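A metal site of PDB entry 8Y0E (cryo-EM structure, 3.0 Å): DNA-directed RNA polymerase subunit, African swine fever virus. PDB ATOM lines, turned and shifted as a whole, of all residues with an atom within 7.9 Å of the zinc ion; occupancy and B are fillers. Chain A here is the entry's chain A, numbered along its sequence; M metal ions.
The zinc ion is bound by the side-chain sulfur (SG) of Cys 134, the side-chain sulfur (SG) of Cys 99, the side-chain sulfur (SG) of Cys 102 and the side-chain sulfur (SG) of Cys 137. The zinc ion has four donor atoms within binding distance.
The side-chain sulfur (SG) of Cys 134 sits close to the backbone NH (N) of Val 136 (3.8 Å). The backbone carbonyl oxygen (O) of Ala 139 is in hydrogen-bond range of the backbone NH (N) of Cys 134, at 3.1 Å. The side-chain sulfur of Cys 99 sits close to the backbone NH of Asn 101 (3.4 Å). The backbone carbonyl oxygen (O) of Ala 104 sits close to the backbone NH (N) of Cys 99, at 3.4 Å. N of Ala 104 sits close to SG of Cys 102 (3.3 Å). SG of Cys 137 sits close to N of Ala 139, at 3.6 Å.
Within 4 Å of the zinc ion: Cys 99, Cys 102, Cys 134 and Cys 137. The nearest printed residue that does not touch the zinc ion is Val 136 (4.4 Å).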
ATOM      1  N   ILE A  98       7.361 -13.183 -13.681  1.00  0.00           N
ATOM      2  CA  ILE A  98       7.187 -12.846 -15.088  1.00  0.00           C
ATOM      3  C   ILE A  98       7.029 -11.341 -15.268  1.00  0.00           C
ATOM      4  O   ILE A  98       6.532 -10.622 -14.384  1.00  0.00           O
ATOM      5  CB  ILE A  98       5.992 -13.619 -15.678  1.00  0.00           C
ATOM      6  CG1 ILE A  98       6.137 -13.727 -17.196  1.00  0.00           C
ATOM      7  CG2 ILE A  98       4.676 -12.956 -15.320  1.00  0.00           C
ATOM      8  CD1 ILE A  98       5.454 -14.926 -17.772  1.00  0.00           C
ATOM      9  N   CYS A  99       7.481 -10.854 -16.425  1.00  0.00           N
ATOM     10  CA  CYS A  99       7.337  -9.456 -16.792  1.00  0.00           C
ATOM     11  C   CYS A  99       5.878  -9.139 -17.093  1.00  0.00           C
ATOM     12  O   CYS A  99       5.186  -9.889 -17.786  1.00  0.00           O
ATOM     13  CB  CYS A  99       8.206  -9.140 -18.015  1.00  0.00           C
ATOM     14  SG  CYS A  99       7.833  -7.585 -18.859  1.00  0.00           S
ATOM     15  N   LEU A 100       5.422  -8.001 -16.575  1.00  0.00           N
ATOM     16  CA  LEU A 100       4.020  -7.627 -16.640  1.00  0.00           C
ATOM     17  C   LEU A 100       3.640  -6.913 -17.931  1.00  0.00           C
ATOM     18  O   LEU A 100       2.479  -6.520 -18.080  1.00  0.00           O
ATOM     19  CB  LEU A 100       3.655  -6.748 -15.436  1.00  0.00           C
ATOM     20  CG  LEU A 100       3.439  -7.456 -14.098  1.00  0.00           C
ATOM     21  CD1 LEU A 100       4.774  -7.768 -13.433  1.00  0.00           C
ATOM     22  CD2 LEU A 100       2.588  -6.605 -13.191  1.00  0.00           C
ATOM     23  N   ASN A 101       4.577  -6.741 -18.859  1.00  0.00           N
ATOM     24  CA  ASN A 101       4.320  -5.928 -20.045  1.00  0.00           C
ATOM     25  C   ASN A 101       4.355  -6.712 -21.353  1.00  0.00           C
ATOM     26  O   ASN A 101       3.831  -6.214 -22.353  1.00  0.00           O
ATOM     27  CB  ASN A 101       5.344  -4.788 -20.137  1.00  0.00           C
ATOM     28  CG  ASN A 101       4.699  -3.427 -20.035  1.00  0.00           C
ATOM     29  OD1 ASN A 101       3.498  -3.279 -20.263  1.00  0.00           O
ATOM     30  ND2 ASN A 101       5.486  -2.422 -19.692  1.00  0.00           N
ATOM     31  N   CYS A 102       4.951  -7.897 -21.372  1.00  0.00           N
ATOM     32  CA  CYS A 102       5.027  -8.661 -22.620  1.00  0.00           C
ATOM     33  C   CYS A 102       4.704 -10.133 -22.490  1.00  0.00           C
ATOM     34  O   CYS A 102       4.464 -10.786 -23.519  1.00  0.00           O
ATOM     35  CB  CYS A 102       6.419  -8.514 -23.247  1.00  0.00           C
ATOM     36  SG  CYS A 102       7.726  -9.312 -22.310  1.00  0.00           S
ATOM     37  N   GLY A 103       4.682 -10.706 -21.287  1.00  0.00           N
ATOM     38  CA  GLY A 103       4.464 -12.121 -21.130  1.00  0.00           C
ATOM     39  C   GLY A 103       5.700 -12.982 -21.251  1.00  0.00           C
ATOM     40  O   GLY A 103       5.583 -14.215 -21.221  1.00  0.00           O
ATOM     41  N   ALA A 104       6.857 -12.401 -21.386  1.00  0.00           N
ATOM     42  CA  ALA A 104       8.059 -13.208 -21.386  1.00  0.00           C
ATOM     43  C   ALA A 104       8.710 -13.200 -20.011  1.00  0.00           C
ATOM     44  O   ALA A 104       8.665 -12.193 -19.293  1.00  0.00           O
ATOM     45  CB  ALA A 104       9.065 -12.693 -22.425  1.00  0.00           C
ATOM     46  N   PRO A 105       9.316 -14.318 -19.595  1.00  0.00           N
ATOM     47  CA  PRO A 105       9.927 -14.365 -18.274  1.00  0.00           C
ATOM     48  C   PRO A 105      11.214 -13.558 -18.233  1.00  0.00           C
ATOM     49  O   PRO A 105      11.996 -13.564 -19.190  1.00  0.00           O
ATOM     50  CB  PRO A 105      10.205 -15.853 -18.066  1.00  0.00           C
ATOM     51  CG  PRO A 105      10.422 -16.366 -19.445  1.00  0.00           C
ATOM     52  CD  PRO A 105       9.516 -15.570 -20.339  1.00  0.00           C
ATOM     53  N   ILE A 106      11.440 -12.870 -17.116  1.00  0.00           N
ATOM     54  CA  ILE A 106      12.650 -12.078 -16.941  1.00  0.00           C
ATOM     55  C   ILE A 106      13.671 -12.764 -16.036  1.00  0.00           C
ATOM     56  O   ILE A 106      14.817 -12.282 -15.940  1.00  0.00           O
ATOM     57  CB  ILE A 106      12.320 -10.653 -16.467  1.00  0.00           C
ATOM     58  CG1 ILE A 106      11.435 -10.615 -15.207  1.00  0.00           C
ATOM     59  CG2 ILE A 106      11.645  -9.882 -17.565  1.00  0.00           C
ATOM     60  CD1 ILE A 106      12.040 -11.148 -13.945  1.00  0.00           C
ATOM     61  N   GLN A 133      15.068  -5.578 -15.422  1.00  0.00           N
ATOM     62  CA  GLN A 133      14.673  -5.102 -16.738  1.00  0.00           C
ATOM     63  C   GLN A 133      14.405  -6.286 -17.664  1.00  0.00           C
ATOM     64  O   GLN A 133      15.095  -7.312 -17.578  1.00  0.00           O
ATOM     65  CB  GLN A 133      15.756  -4.205 -17.340  1.00  0.00           C
ATOM     66  CG  GLN A 133      15.259  -3.278 -18.428  1.00  0.00           C
ATOM     67  CD  GLN A 133      16.239  -2.160 -18.723  1.00  0.00           C
ATOM     68  OE1 GLN A 133      17.453  -2.358 -18.691  1.00  0.00           O
ATOM     69  NE2 GLN A 133      15.719  -0.970 -19.013  1.00  0.00           N
ATOM     70  N   CYS A 134      13.405  -6.141 -18.520  1.00  0.00           N
ATOM     71  CA  CYS A 134      13.094  -7.200 -19.474  1.00  0.00           C
ATOM     72  C   CYS A 134      14.084  -7.208 -20.616  1.00  0.00           C
ATOM     73  O   CYS A 134      14.659  -6.173 -20.987  1.00  0.00           O
ATOM     74  CB  CYS A 134      11.668  -7.029 -20.013  1.00  0.00           C
ATOM     75  SG  CYS A 134      11.016  -8.511 -20.797  1.00  0.00           S
ATOM     76  N   TYR A 135      14.289  -8.384 -21.193  1.00  0.00           N
ATOM     77  CA  TYR A 135      15.259  -8.567 -22.262  1.00  0.00           C
ATOM     78  C   TYR A 135      14.661  -8.477 -23.661  1.00  0.00           C
ATOM     79  O   TYR A 135      15.406  -8.507 -24.643  1.00  0.00           O
ATOM     80  CB  TYR A 135      15.980  -9.905 -22.104  1.00  0.00           C
ATOM     81  CG  TYR A 135      16.396 -10.219 -20.683  1.00  0.00           C
ATOM     82  CD1 TYR A 135      17.452  -9.535 -20.084  1.00  0.00           C
ATOM     83  CD2 TYR A 135      15.748 -11.198 -19.944  1.00  0.00           C
ATOM     84  CE1 TYR A 135      17.840  -9.815 -18.791  1.00  0.00           C
ATOM     85  CE2 TYR A 135      16.119 -11.481 -18.647  1.00  0.00           C
ATOM     86  CZ  TYR A 135      17.167 -10.791 -18.075  1.00  0.00           C
ATOM     87  OH  TYR A 135      17.542 -11.075 -16.786  1.00  0.00           O
ATOM     88  N   VAL A 136      13.337  -8.363 -23.784  1.00  0.00           N
ATOM     89  CA  VAL A 136      12.701  -8.249 -25.083  1.00  0.00           C
ATOM     90  C   VAL A 136      11.862  -6.986 -25.237  1.00  0.00           C
ATOM     91  O   VAL A 136      11.642  -6.542 -26.372  1.00  0.00           O
ATOM     92  CB  VAL A 136      11.850  -9.492 -25.406  1.00  0.00           C
ATOM     93  CG1 VAL A 136      12.730 -10.723 -25.537  1.00  0.00           C
ATOM     94  CG2 VAL A 136      10.785  -9.699 -24.341  1.00  0.00           C
ATOM     95  N   CYS A 137      11.380  -6.400 -24.138  1.00  0.00           N
ATOM     96  CA  CYS A 137      10.618  -5.160 -24.200  1.00  0.00           C
ATOM     97  C   CYS A 137      11.196  -4.061 -23.335  1.00  0.00           C
ATOM     98  O   CYS A 137      10.641  -2.953 -23.308  1.00  0.00           O
ATOM     99  CB  CYS A 137       9.154  -5.413 -23.809  1.00  0.00           C
ATOM    100  SG  CYS A 137       8.883  -5.705 -22.053  1.00  0.00           S
ATOM    101  N   LYS A 138      12.292  -4.324 -22.617  1.00  0.00           N
ATOM    102  CA  LYS A 138      13.031  -3.358 -21.814  1.00  0.00           C
ATOM    103  C   LYS A 138      12.184  -2.724 -20.707  1.00  0.00           C
ATOM    104  O   LYS A 138      12.609  -1.719 -20.125  1.00  0.00           O
ATOM    105  CB  LYS A 138      13.652  -2.256 -22.683  1.00  0.00           C
ATOM    106  CG  LYS A 138      14.393  -2.774 -23.900  1.00  0.00           C
ATOM    107  CD  LYS A 138      15.449  -3.801 -23.533  1.00  0.00           C
ATOM    108  CE  LYS A 138      16.572  -3.186 -22.729  1.00  0.00           C
ATOM    109  NZ  LYS A 138      17.703  -4.147 -22.582  1.00  0.00           N
ATOM    110  N   ALA A 139      11.025  -3.281 -20.400  1.00  0.00           N
ATOM    111  CA  ALA A 139      10.201  -2.757 -19.331  1.00  0.00           C
ATOM    112  C   ALA A 139      10.754  -3.191 -17.986  1.00  0.00           C
ATOM    113  O   ALA A 139      11.008  -4.388 -17.767  1.00  0.00           O
ATOM    114  CB  ALA A 139       8.753  -3.229 -19.483  1.00  0.00           C
ATOM    115  N   VAL A 140      10.954  -2.229 -17.088  1.00  0.00           N
ATOM    116  CA  VAL A 140      11.471  -2.565 -15.763  1.00  0.00           C
ATOM    117  C   VAL A 140      10.393  -3.276 -14.956  1.00  0.00           C
ATOM    118  O   VAL A 140       9.186  -3.111 -15.201  1.00  0.00           O
ATOM    119  CB  VAL A 140      11.970  -1.293 -15.047  1.00  0.00           C
ATOM    120  CG1 VAL A 140      10.849  -0.598 -14.311  1.00  0.00           C
ATOM    121  CG2 VAL A 140      13.105  -1.625 -14.091  1.00  0.00           C
HETATM  122 ZN    ZN M   1       8.825  -7.767 -20.954  1.00  0.00          ZN
